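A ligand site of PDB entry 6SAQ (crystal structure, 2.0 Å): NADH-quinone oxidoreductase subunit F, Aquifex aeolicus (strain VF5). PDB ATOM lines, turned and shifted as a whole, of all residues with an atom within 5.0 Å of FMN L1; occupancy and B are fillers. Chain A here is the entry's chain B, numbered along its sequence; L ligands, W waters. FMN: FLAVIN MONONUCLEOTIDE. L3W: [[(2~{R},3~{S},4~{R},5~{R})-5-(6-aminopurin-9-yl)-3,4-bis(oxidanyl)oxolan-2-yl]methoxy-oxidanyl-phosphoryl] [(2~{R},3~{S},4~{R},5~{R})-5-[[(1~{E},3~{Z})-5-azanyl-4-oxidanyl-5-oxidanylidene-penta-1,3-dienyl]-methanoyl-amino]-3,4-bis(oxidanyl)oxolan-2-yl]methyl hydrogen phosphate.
An oxygen (O1P) of FMN L1 lies within salt-bridge range of the side-chain amino group (NZ) of Lys 76, at 2.8 Å. O52 of L3W L2 is in hydrogen-bond range of NZ of Lys 76 (2.9 Å). N of Asn 220 lies within hydrogen-bond range of O3P of FMN L1, 2.9 Å away. ND2 of Asn 219 sits at hydrogen-bond distance from O3P of FMN L1 (2.9 Å). N of Glu 185 lies within hydrogen-bond range of O2' of FMN L1, at 3.0 Å. An oxygen (O3P) of FMN L1 sits at hydrogen-bond distance from the side-chain hydroxyl of Thr 223 (2.7 Å). O51 of L3W L2 sits at hydrogen-bond distance from O of Gly 68 (3.4 Å). O of Gly 67 lies within hydrogen-bond range of O47 of L3W L2, 2.7 Å away. An oxygen (O45) of L3W L2 is in hydrogen-bond range of the backbone NH (N) of Ser 96 (3.5 Å). O4' of FMN L1 is in hydrogen-bond range of ND2 of Asn 92 (3.1 Å). O4 of FMN L1 sits at hydrogen-bond distance from N of Glu 95 (3.0 Å). An oxygen (O2P) of FMN L1 sits at hydrogen-bond distance from the backbone NH (N) of Arg 66, at 3.4 Å. O2 of FMN L1 lies within hydrogen-bond range of ND2 of Asn 220 (2.8 Å). The side-chain amino group of Lys 202 is in salt-bridge range of an oxygen (O27) of L3W L2. The side-chain carboxylate (OE2) of Glu 185 lies within hydrogen-bond range of an oxygen (O53) of L3W L2 (2.6 Å). The side-chain carboxylate of Glu 95 is in hydrogen-bond range of a nitrogen (N46) of L3W L2 (3.5 Å). The backbone NH (N) of Gly 67 lies within hydrogen-bond range of an oxygen (O2P) of FMN L1 (2.8 Å). The side-chain carboxylate (OD2) of Asp 103 is in hydrogen-bond range of a nitrogen (N46) of L3W L2 (2.9 Å).
An oxygen (O27) of L3W L2 sits at hydrogen-bond distance from an oxygen (O2') of FMN L1 (2.8 Å).
The side-chain amino group (NZ) of Lys 202 is in salt-bridge range of the side-chain carboxylate (OE2) of Glu 185, at 2.8 Å. The side-chain hydroxyl (OG) of Ser 96 is in hydrogen-bond range of the backbone carbonyl oxygen (O) of Asp 94, 2.8 Å away. The side-chain carboxylate (OD2) of Asp 94 lies within hydrogen-bond range of the backbone NH (N) of Gly 183 (3.2 Å). The backbone NH (N) of Gly 65 is in hydrogen-bond range of the backbone carbonyl oxygen (O) of Phe 71 (2.9 Å). O of Asn 219 sits at hydrogen-bond distance from N of Asn 92 (2.7 Å). NZ of Lys 202 is in salt-bridge range of OE2 of Glu 184 (3.4 Å). The side-chain amide nitrogen of Asn 92 sits at hydrogen-bond distance from the backbone carbonyl oxygen of Gly 183, 2.8 Å away. The backbone NH of Arg 66 is in hydrogen-bond range of the side-chain hydroxyl of Thr 223, at 2.8 Å.
O of Gly 183 lies close to N10 of FMN L1 (3.3 Å). Gly 65 touches FMN L1 (CA to O2P, 3.3 Å). C of Asp 94 touches O4 of FMN L1, 3.5 Å away. N of Ser 96 touches O4 of FMN L1 (3.7 Å). CE2 of Tyr 180 touches C7M of FMN L1, at 3.6 Å. Ile 181 touches FMN L1. Glu 184 touches FMN L1 (N to C5A, 3.6 Å). Val 218 touches FMN L1. Gly 394 touches FMN L1 (CA to C8M, 3.8 Å). Hydrophobic or aromatic side chains within 4 Å of FMN L1: Tyr 180, Ile 181 and Val 218. 18 residues have an atom within 4 Å of FMN L1: Gly 65, Arg 66, Gly 67, Lys 76, Asn 92, Asp 94, Glu 95, Ser 96, Tyr 180, Ile 181, Gly 183, Glu 184, Glu 185, Val 218, Asn 219, Asn 220, Thr 223 and Gly 394. The nearest printed residue that does not touch FMN L1 is Leu 395 (4.01 Å).
Water W3 lies within hydrogen-bond range of an oxygen (O1P) of FMN L1 (2.7 Å), the backbone carbonyl oxygen (O) of Phe 71 (2.8 Å), the side-chain amide nitrogen (ND2) of Asn 219 (3.2 Å) and the backbone NH (N) of Gly 65 (3.5 Å). Water W4 lies within hydrogen-bond range of an oxygen (O1P) of FMN L1 (2.7 Å) and the backbone NH of Phe 71 (3.0 Å). Water W5 lies within hydrogen-bond range of an oxygen (O2P) of FMN L1 (2.7 Å), the backbone NH of Ala 69 (2.9 Å) and the backbone NH of Gly 68 (3.4 Å).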
ATOM      1  N   GLY A  65     -21.709 -26.986  10.682  1.00  0.00           N
ATOM      2  CA  GLY A  65     -22.250 -25.638  10.713  1.00  0.00           C
ATOM      3  C   GLY A  65     -21.218 -24.574  10.991  1.00  0.00           C
ATOM      4  O   GLY A  65     -20.529 -24.620  12.018  1.00  0.00           O
ATOM      5  N   ARG A  66     -21.082 -23.632  10.063  1.00  0.00           N
ATOM      6  CA  ARG A  66     -20.106 -22.531  10.104  1.00  0.00           C
ATOM      7  C   ARG A  66     -20.665 -21.294  10.843  1.00  0.00           C
ATOM      8  O   ARG A  66     -19.976 -20.281  10.949  1.00  0.00           O
ATOM      9  CB  ARG A  66     -19.674 -22.173   8.651  1.00  0.00           C
ATOM     10  CG  ARG A  66     -19.110 -23.365   7.811  1.00  0.00           C
ATOM     11  CD  ARG A  66     -17.895 -24.040   8.446  1.00  0.00           C
ATOM     12  NE  ARG A  66     -17.028 -24.701   7.463  1.00  0.00           N
ATOM     13  CZ  ARG A  66     -16.716 -25.991   7.476  1.00  0.00           C
ATOM     14  NH1 ARG A  66     -15.876 -26.475   6.566  1.00  0.00           N
ATOM     15  NH2 ARG A  66     -17.201 -26.796   8.415  1.00  0.00           N
ATOM     16  N   GLY A  67     -21.905 -21.390  11.329  1.00  0.00           N
ATOM     17  CA  GLY A  67     -22.549 -20.327  12.104  1.00  0.00           C
ATOM     18  C   GLY A  67     -22.044 -20.243  13.544  1.00  0.00           C
ATOM     19  O   GLY A  67     -22.395 -19.313  14.258  1.00  0.00           O
ATOM     20  N   GLY A  68     -21.223 -21.208  13.968  1.00  0.00           N
ATOM     21  CA  GLY A  68     -20.619 -21.189  15.299  1.00  0.00           C
ATOM     22  C   GLY A  68     -20.770 -22.442  16.148  1.00  0.00           C
ATOM     23  O   GLY A  68     -19.893 -22.709  16.965  1.00  0.00           O
ATOM     24  N   ALA A  69     -21.879 -23.213  15.984  1.00  0.00           N
ATOM     25  CA  ALA A  69     -22.070 -24.417  16.829  1.00  0.00           C
ATOM     26  C   ALA A  69     -21.438 -25.692  16.261  1.00  0.00           C
ATOM     27  O   ALA A  69     -21.276 -26.655  16.994  1.00  0.00           O
ATOM     28  CB  ALA A  69     -23.549 -24.628  17.135  1.00  0.00           C
ATOM     29  N   PHE A  71     -22.723 -27.955  14.196  1.00  0.00           N
ATOM     30  CA  PHE A  71     -23.598 -29.143  14.102  1.00  0.00           C
ATOM     31  C   PHE A  71     -23.441 -29.788  12.694  1.00  0.00           C
ATOM     32  O   PHE A  71     -23.426 -29.038  11.709  1.00  0.00           O
ATOM     33  CB  PHE A  71     -25.089 -28.792  14.373  1.00  0.00           C
ATOM     34  CG  PHE A  71     -25.999 -29.991  14.572  1.00  0.00           C
ATOM     35  CD1 PHE A  71     -26.670 -30.574  13.491  1.00  0.00           C
ATOM     36  CD2 PHE A  71     -26.149 -30.569  15.828  1.00  0.00           C
ATOM     37  CE1 PHE A  71     -27.461 -31.724  13.663  1.00  0.00           C
ATOM     38  CE2 PHE A  71     -26.947 -31.716  16.013  1.00  0.00           C
ATOM     39  CZ  PHE A  71     -27.619 -32.262  14.939  1.00  0.00           C
ATOM     40  N   LYS A  76     -28.404 -32.603  10.131  1.00  0.00           N
ATOM     41  CA  LYS A  76     -29.502 -31.651  10.328  1.00  0.00           C
ATOM     42  C   LYS A  76     -30.575 -31.822   9.196  1.00  0.00           C
ATOM     43  O   LYS A  76     -31.765 -31.850   9.474  1.00  0.00           O
ATOM     44  CB  LYS A  76     -28.963 -30.210  10.301  1.00  0.00           C
ATOM     45  CG  LYS A  76     -30.032 -29.178  10.689  1.00  0.00           C
ATOM     46  CD  LYS A  76     -29.558 -27.739  10.472  1.00  0.00           C
ATOM     47  CE  LYS A  76     -28.375 -27.348  11.334  1.00  0.00           C
ATOM     48  NZ  LYS A  76     -28.169 -25.880  11.289  1.00  0.00           N
ATOM     49  N   ASN A  92     -29.066 -18.059   6.986  1.00  0.00           N
ATOM     50  CA  ASN A  92     -28.841 -17.103   8.060  1.00  0.00           C
ATOM     51  C   ASN A  92     -27.683 -16.148   7.658  1.00  0.00           C
ATOM     52  O   ASN A  92     -26.512 -16.529   7.702  1.00  0.00           O
ATOM     53  CB  ASN A  92     -28.544 -17.850   9.381  1.00  0.00           C
ATOM     54  CG  ASN A  92     -28.563 -16.940  10.592  1.00  0.00           C
ATOM     55  OD1 ASN A  92     -28.426 -15.728  10.487  1.00  0.00           O
ATOM     56  ND2 ASN A  92     -28.753 -17.516  11.765  1.00  0.00           N
ATOM     57  N   ASP A  94     -27.524 -13.029   9.146  1.00  0.00           N
ATOM     58  CA  ASP A  94     -27.614 -11.999  10.183  1.00  0.00           C
ATOM     59  C   ASP A  94     -26.245 -11.463  10.646  1.00  0.00           C
ATOM     60  O   ASP A  94     -26.185 -10.353  11.145  1.00  0.00           O
ATOM     61  CB  ASP A  94     -28.437 -12.448  11.402  1.00  0.00           C
ATOM     62  CG  ASP A  94     -28.866 -11.233  12.215  1.00  0.00           C
ATOM     63  OD1 ASP A  94     -29.645 -10.405  11.682  1.00  0.00           O
ATOM     64  OD2 ASP A  94     -28.350 -11.066  13.371  1.00  0.00           O
ATOM     65  N   GLU A  95     -25.179 -12.270  10.552  1.00  0.00           N
ATOM     66  CA  GLU A  95     -23.815 -11.921  10.943  1.00  0.00           C
ATOM     67  C   GLU A  95     -23.680 -10.649  11.815  1.00  0.00           C
ATOM     68  O   GLU A  95     -23.337  -9.570  11.310  1.00  0.00           O
ATOM     69  CB  GLU A  95     -22.932 -11.801   9.701  1.00  0.00           C
ATOM     70  CG  GLU A  95     -21.484 -11.483  10.032  1.00  0.00           C
ATOM     71  CD  GLU A  95     -20.539 -11.907   8.941  1.00  0.00           C
ATOM     72  OE1 GLU A  95     -20.426 -11.175   7.927  1.00  0.00           O
ATOM     73  OE2 GLU A  95     -19.930 -12.977   9.082  1.00  0.00           O
ATOM     74  N   SER A  96     -23.945 -10.768  13.129  1.00  0.00           N
ATOM     75  CA  SER A  96     -23.848  -9.616  14.026  1.00  0.00           C
ATOM     76  C   SER A  96     -22.937  -9.861  15.219  1.00  0.00           C
ATOM     77  O   SER A  96     -22.882  -9.030  16.141  1.00  0.00           O
ATOM     78  CB  SER A  96     -25.235  -9.168  14.494  1.00  0.00           C
ATOM     79  OG  SER A  96     -25.949  -8.634  13.393  1.00  0.00           O
ATOM     80  N   ASP A 103     -19.116 -13.764   6.484  1.00  0.00           N
ATOM     81  CA  ASP A 103     -20.263 -14.045   5.615  1.00  0.00           C
ATOM     82  C   ASP A 103     -20.498 -12.962   4.572  1.00  0.00           C
ATOM     83  O   ASP A 103     -20.838 -13.292   3.437  1.00  0.00           O
ATOM     84  CB  ASP A 103     -21.543 -14.286   6.450  1.00  0.00           C
ATOM     85  CG  ASP A 103     -21.438 -15.458   7.430  1.00  0.00           C
ATOM     86  OD1 ASP A 103     -20.634 -16.379   7.176  1.00  0.00           O
ATOM     87  OD2 ASP A 103     -22.181 -15.463   8.422  1.00  0.00           O
ATOM     88  N   TYR A 180     -28.983  -8.242  17.278  1.00  0.00           N
ATOM     89  CA  TYR A 180     -28.050  -9.380  17.258  1.00  0.00           C
ATOM     90  C   TYR A 180     -28.775 -10.691  17.562  1.00  0.00           C
ATOM     91  O   TYR A 180     -28.425 -11.741  17.013  1.00  0.00           O
ATOM     92  CB  TYR A 180     -26.993  -9.152  18.348  1.00  0.00           C
ATOM     93  CG  TYR A 180     -26.182 -10.363  18.738  1.00  0.00           C
ATOM     94  CD1 TYR A 180     -25.298 -10.954  17.848  1.00  0.00           C
ATOM     95  CD2 TYR A 180     -26.258 -10.885  20.032  1.00  0.00           C
ATOM     96  CE1 TYR A 180     -24.495 -12.023  18.230  1.00  0.00           C
ATOM     97  CE2 TYR A 180     -25.462 -11.951  20.426  1.00  0.00           C
ATOM     98  CZ  TYR A 180     -24.574 -12.521  19.525  1.00  0.00           C
ATOM     99  OH  TYR A 180     -23.764 -13.555  19.902  1.00  0.00           O
ATOM    100  N   ILE A 181     -29.818 -10.632  18.410  1.00  0.00           N
ATOM    101  CA  ILE A 181     -30.569 -11.840  18.773  1.00  0.00           C
ATOM    102  C   ILE A 181     -31.293 -12.454  17.567  1.00  0.00           C
ATOM    103  O   ILE A 181     -31.574 -13.642  17.597  1.00  0.00           O
ATOM    104  CB  ILE A 181     -31.502 -11.591  19.991  1.00  0.00           C
ATOM    105  CG1 ILE A 181     -31.965 -12.926  20.667  1.00  0.00           C
ATOM    106  CG2 ILE A 181     -32.695 -10.675  19.628  1.00  0.00           C
ATOM    107  CD1 ILE A 181     -30.868 -13.845  21.084  1.00  0.00           C
ATOM    108  N   GLY A 183     -30.015 -13.308  14.941  1.00  0.00           N
ATOM    109  CA  GLY A 183     -29.075 -14.285  14.429  1.00  0.00           C
ATOM    110  C   GLY A 183     -29.362 -15.656  15.009  1.00  0.00           C
ATOM    111  O   GLY A 183     -29.025 -16.677  14.394  1.00  0.00           O
ATOM    112  N   GLU A 184     -29.963 -15.705  16.223  1.00  0.00           N
ATOM    113  CA  GLU A 184     -30.347 -16.974  16.886  1.00  0.00           C
ATOM    114  C   GLU A 184     -31.489 -17.521  16.030  1.00  0.00           C
ATOM    115  O   GLU A 184     -32.424 -16.781  15.747  1.00  0.00           O
ATOM    116  CB  GLU A 184     -30.753 -16.747  18.355  1.00  0.00           C
ATOM    117  CG  GLU A 184     -30.767 -17.994  19.225  1.00  0.00           C
ATOM    118  CD  GLU A 184     -32.030 -18.838  19.173  1.00  0.00           C
ATOM    119  OE1 GLU A 184     -33.049 -18.355  18.638  1.00  0.00           O
ATOM    120  OE2 GLU A 184     -32.003 -19.978  19.686  1.00  0.00           O
ATOM    121  N   GLU A 185     -31.353 -18.742  15.524  1.00  0.00           N
ATOM    122  CA  GLU A 185     -32.273 -19.291  14.505  1.00  0.00           C
ATOM    123  C   GLU A 185     -33.764 -19.228  14.834  1.00  0.00           C
ATOM    124  O   GLU A 185     -34.544 -19.038  13.901  1.00  0.00           O
ATOM    125  CB  GLU A 185     -31.901 -20.720  14.118  1.00  0.00           C
ATOM    126  CG  GLU A 185     -31.980 -21.647  15.321  1.00  0.00           C
ATOM    127  CD  GLU A 185     -31.732 -23.100  15.052  1.00  0.00           C
ATOM    128  OE1 GLU A 185     -31.387 -23.432  13.894  1.00  0.00           O
ATOM    129  OE2 GLU A 185     -31.878 -23.900  16.005  1.00  0.00           O
ATOM    130  N   LYS A 202     -36.292 -24.533  22.864  1.00  0.00           N
ATOM    131  CA  LYS A 202     -35.782 -25.632  22.019  1.00  0.00           C
ATOM    132  C   LYS A 202     -35.381 -26.813  22.933  1.00  0.00           C
ATOM    133  O   LYS A 202     -34.669 -26.564  23.897  1.00  0.00           O
ATOM    134  CB  LYS A 202     -34.542 -25.220  21.208  1.00  0.00           C
ATOM    135  CG  LYS A 202     -34.715 -24.154  20.132  1.00  0.00           C
ATOM    136  CD  LYS A 202     -33.392 -23.366  19.870  1.00  0.00           C
ATOM    137  CE  LYS A 202     -32.321 -24.058  19.034  1.00  0.00           C
ATOM    138  NZ  LYS A 202     -31.192 -23.142  18.609  1.00  0.00           N
ATOM    139  N   VAL A 218     -32.273 -24.160   9.024  1.00  0.00           N
ATOM    140  CA  VAL A 218     -31.575 -22.890   9.069  1.00  0.00           C
ATOM    141  C   VAL A 218     -30.088 -23.234   8.970  1.00  0.00           C
ATOM    142  O   VAL A 218     -29.591 -24.053   9.763  1.00  0.00           O
ATOM    143  CB  VAL A 218     -31.869 -22.013  10.327  1.00  0.00           C
ATOM    144  CG1 VAL A 218     -31.080 -20.695  10.295  1.00  0.00           C
ATOM    145  CG2 VAL A 218     -33.370 -21.737  10.468  1.00  0.00           C
ATOM    146  N   ASN A 219     -29.382 -22.631   8.004  1.00  0.00           N
ATOM    147  CA  ASN A 219     -27.936 -22.781   7.873  1.00  0.00           C
ATOM    148  C   ASN A 219     -27.314 -21.434   7.642  1.00  0.00           C
ATOM    149  O   ASN A 219     -27.928 -20.546   7.048  1.00  0.00           O
ATOM    150  CB  ASN A 219     -27.525 -23.743   6.723  1.00  0.00           C
ATOM    151  CG  ASN A 219     -27.498 -25.212   7.092  1.00  0.00           C
ATOM    152  OD1 ASN A 219     -28.152 -26.027   6.460  1.00  0.00           O
ATOM    153  ND2 ASN A 219     -26.721 -25.589   8.089  1.00  0.00           N
ATOM    154  N   ASN A 220     -26.065 -21.296   8.103  1.00  0.00           N
ATOM    155  CA  ASN A 220     -25.264 -20.093   7.947  1.00  0.00           C
ATOM    156  C   ASN A 220     -24.794 -19.952   6.480  1.00  0.00           C
ATOM    157  O   ASN A 220     -24.624 -20.951   5.786  1.00  0.00           O
ATOM    158  CB  ASN A 220     -24.066 -20.203   8.897  1.00  0.00           C
ATOM    159  CG  ASN A 220     -23.032 -19.139   8.714  1.00  0.00           C
ATOM    160  OD1 ASN A 220     -21.993 -19.390   8.140  1.00  0.00           O
ATOM    161  ND2 ASN A 220     -23.293 -17.935   9.217  1.00  0.00           N
ATOM    162  N   THR A 223     -21.703 -22.089   5.615  1.00  0.00           N
ATOM    163  CA  THR A 223     -22.052 -23.510   5.497  1.00  0.00           C
ATOM    164  C   THR A 223     -22.620 -23.770   4.073  1.00  0.00           C
ATOM    165  O   THR A 223     -22.189 -24.688   3.387  1.00  0.00           O
ATOM    166  CB  THR A 223     -23.082 -23.907   6.546  1.00  0.00           C
ATOM    167  OG1 THR A 223     -22.687 -23.407   7.831  1.00  0.00           O
ATOM    168  CG2 THR A 223     -23.312 -25.423   6.599  1.00  0.00           C
ATOM    169  N   CYS A 393     -32.117 -19.366  25.491  1.00  0.00           N
ATOM    170  CA  CYS A 393     -31.281 -19.331  24.301  1.00  0.00           C
ATOM    171  C   CYS A 393     -29.786 -19.206  24.676  1.00  0.00           C
ATOM    172  O   CYS A 393     -29.462 -19.023  25.849  1.00  0.00           O
ATOM    173  CB  CYS A 393     -31.743 -18.296  23.272  1.00  0.00           C
ATOM    174  SG  CYS A 393     -30.897 -16.696  23.378  1.00  0.00           S
ATOM    175  N   GLY A 394     -28.910 -19.336  23.680  1.00  0.00           N
ATOM    176  CA  GLY A 394     -27.466 -19.289  23.851  1.00  0.00           C
ATOM    177  C   GLY A 394     -26.897 -17.966  24.344  1.00  0.00           C
ATOM    178  O   GLY A 394     -25.822 -17.961  24.930  1.00  0.00           O
ATOM    179  N   LEU A 395     -27.609 -16.844  24.137  1.00  0.00           N
ATOM    180  CA  LEU A 395     -27.123 -15.542  24.620  1.00  0.00           C
ATOM    181  C   LEU A 395     -26.986 -15.511  26.176  1.00  0.00           C
ATOM    182  O   LEU A 395     -25.915 -15.171  26.681  1.00  0.00           O
ATOM    183  CB  LEU A 395     -27.974 -14.376  24.101  1.00  0.00           C
ATOM    184  CG  LEU A 395     -27.401 -12.943  24.290  1.00  0.00           C
ATOM    185  CD1 LEU A 395     -27.981 -11.995  23.280  1.00  0.00           C
ATOM    186  CD2 LEU A 395     -27.677 -12.381  25.741  1.00  0.00           C
HETATM  187  N1  FMN L   1     -25.753 -18.175  13.176  1.00  0.00           N
HETATM  188  C2  FMN L   1     -25.534 -17.522  12.000  1.00  0.00           C
HETATM  189  O2  FMN L   1     -25.514 -18.140  10.925  1.00  0.00           O
HETATM  190  N3  FMN L   1     -25.438 -16.136  11.977  1.00  0.00           N
HETATM  191  C4  FMN L   1     -25.587 -15.289  13.060  1.00  0.00           C
HETATM  192  O4  FMN L   1     -25.471 -14.078  12.918  1.00  0.00           O
HETATM  193  C4A FMN L   1     -25.850 -15.998  14.325  1.00  0.00           C
HETATM  194  N5  FMN L   1     -26.061 -15.288  15.398  1.00  0.00           N
HETATM  195  C5A FMN L   1     -26.386 -15.961  16.583  1.00  0.00           C
HETATM  196  C6  FMN L   1     -26.665 -15.215  17.733  1.00  0.00           C
HETATM  197  C7  FMN L   1     -27.003 -15.840  18.940  1.00  0.00           C
HETATM  198  C7M FMN L   1     -27.344 -14.991  20.144  1.00  0.00           C
HETATM  199  C8  FMN L   1     -27.070 -17.257  18.996  1.00  0.00           C
HETATM  200  C8M FMN L   1     -27.287 -17.987  20.302  1.00  0.00           C
HETATM  201  C9  FMN L   1     -26.817 -17.992  17.837  1.00  0.00           C
HETATM  202  C9A FMN L   1     -26.481 -17.372  16.639  1.00  0.00           C
HETATM  203  N10 FMN L   1     -26.232 -18.099  15.449  1.00  0.00           N
HETATM  204  C10 FMN L   1     -25.912 -17.448  14.275  1.00  0.00           C
HETATM  205  C1' FMN L   1     -26.349 -19.564  15.430  1.00  0.00           C
HETATM  206  C2' FMN L   1     -27.709 -20.028  14.902  1.00  0.00           C
HETATM  207  O2' FMN L   1     -28.651 -20.076  15.981  1.00  0.00           O
HETATM  208  C3' FMN L   1     -27.627 -21.405  14.220  1.00  0.00           C
HETATM  209  O3' FMN L   1     -26.841 -22.301  15.002  1.00  0.00           O
HETATM  210  C4' FMN L   1     -27.048 -21.398  12.802  1.00  0.00           C
HETATM  211  O4' FMN L   1     -27.556 -20.342  11.991  1.00  0.00           O
HETATM  212  C5' FMN L   1     -27.307 -22.721  12.113  1.00  0.00           C
HETATM  213  O5' FMN L   1     -26.476 -22.777  10.945  1.00  0.00           O
HETATM  214  P   FMN L   1     -25.201 -23.741  10.788  1.00  0.00           P
HETATM  215  O1P FMN L   1     -25.515 -25.158  11.296  1.00  0.00           O
HETATM  216  O2P FMN L   1     -24.109 -23.091  11.588  1.00  0.00           O
HETATM  217  O3P FMN L   1     -24.925 -23.678   9.301  1.00  0.00           O
HETATM  218  C1  L3W L   2     -31.818 -31.179  15.283  1.00  0.00           C
HETATM  219  C3  L3W L   2     -30.931 -31.761  17.341  1.00  0.00           C
HETATM  220  N6  L3W L   2     -31.111 -30.054  15.109  1.00  0.00           N
HETATM  221  C8  L3W L   2     -28.793 -28.982  17.514  1.00  0.00           C
HETATM  222  C10 L3W L   2     -29.246 -27.700  15.381  1.00  0.00           C
HETATM  223  C12 L3W L   2     -29.868 -26.397  15.829  1.00  0.00           C
HETATM  224  C14 L3W L   2     -28.963 -25.346  15.160  1.00  0.00           C
HETATM  225  C16 L3W L   2     -27.606 -26.006  15.167  1.00  0.00           C
HETATM  226  C19 L3W L   2     -26.798 -25.618  16.406  1.00  0.00           C
HETATM  227  O28 L3W L   2     -25.884 -21.464  18.302  1.00  0.00           O
HETATM  228  C30 L3W L   2     -23.633 -20.736  18.540  1.00  0.00           C
HETATM  229  C32 L3W L   2     -22.538 -20.369  19.524  1.00  0.00           C
HETATM  230  C34 L3W L   2     -21.824 -19.179  18.899  1.00  0.00           C
HETATM  231  N2  L3W L   2     -31.765 -32.018  16.323  1.00  0.00           N
HETATM  232  C4  L3W L   2     -30.139 -30.622  17.264  1.00  0.00           C
HETATM  233  C5  L3W L   2     -30.293 -29.840  16.138  1.00  0.00           C
HETATM  234  N7  L3W L   2     -29.421 -28.802  16.303  1.00  0.00           N
HETATM  235  N9  L3W L   2     -29.215 -30.080  18.111  1.00  0.00           N
HETATM  236  O18 L3W L   2     -27.873 -27.418  15.188  1.00  0.00           O
HETATM  237  O20 L3W L   2     -27.639 -25.650  17.574  1.00  0.00           O
HETATM  238  P21 L3W L   2     -27.149 -25.290  19.094  1.00  0.00           P
HETATM  239  O22 L3W L   2     -28.443 -25.198  19.869  1.00  0.00           O
HETATM  240  O23 L3W L   2     -26.051 -26.205  19.502  1.00  0.00           O
HETATM  241  O24 L3W L   2     -26.542 -23.789  18.882  1.00  0.00           O
HETATM  242  P25 L3W L   2     -27.238 -22.313  18.720  1.00  0.00           P
HETATM  243  O26 L3W L   2     -27.766 -21.889  20.057  1.00  0.00           O
HETATM  244  O27 L3W L   2     -28.174 -22.309  17.548  1.00  0.00           O
HETATM  245  C29 L3W L   2     -24.860 -21.247  19.257  1.00  0.00           C
HETATM  246  C36 L3W L   2     -22.798 -18.680  17.814  1.00  0.00           C
HETATM  247  O38 L3W L   2     -23.933 -19.547  17.869  1.00  0.00           O
HETATM  248  N39 L3W L   2     -23.367 -17.299  18.004  1.00  0.00           N
HETATM  249  C40 L3W L   2     -22.877 -16.361  17.042  1.00  0.00           C
HETATM  250  C41 L3W L   2     -22.895 -16.591  15.718  1.00  0.00           C
HETATM  251  C42 L3W L   2     -22.492 -15.580  14.770  1.00  0.00           C
HETATM  252  C43 L3W L   2     -22.271 -15.802  13.459  1.00  0.00           C
HETATM  253  C44 L3W L   2     -21.925 -14.615  12.625  1.00  0.00           C
HETATM  254  O45 L3W L   2     -21.805 -13.498  13.090  1.00  0.00           O
HETATM  255  N46 L3W L   2     -21.786 -14.931  11.290  1.00  0.00           N
HETATM  256  O47 L3W L   2     -22.304 -17.021  12.853  1.00  0.00           O
HETATM  257  C48 L3W L   2     -23.349 -16.836  19.378  1.00  0.00           C
HETATM  258  O49 L3W L   2     -23.869 -17.493  20.275  1.00  0.00           O
HETATM  259  O50 L3W L   2     -20.642 -19.631  18.277  1.00  0.00           O
HETATM  260  O51 L3W L   2     -21.699 -21.499  19.564  1.00  0.00           O
HETATM  261  O52 L3W L   2     -29.322 -25.146  13.792  1.00  0.00           O
HETATM  262  O53 L3W L   2     -31.217 -26.296  15.407  1.00  0.00           O
HETATM  263  N54 L3W L   2     -30.873 -32.634  18.443  1.00  0.00           N
HETATM  264  O   HOH W   1     -24.697 -14.986   9.408  1.00  0.00           O
HETATM  265  O   HOH W   2     -26.407 -12.329  14.867  1.00  0.00           O
HETATM  266  O   HOH W   3     -25.079 -27.502  10.029  1.00  0.00           O
HETATM  267  O   HOH W   4     -24.429 -25.570  13.748  1.00  0.00           O
HETATM  268  O   HOH W   5     -24.168 -22.848  14.295  1.00  0.00           O
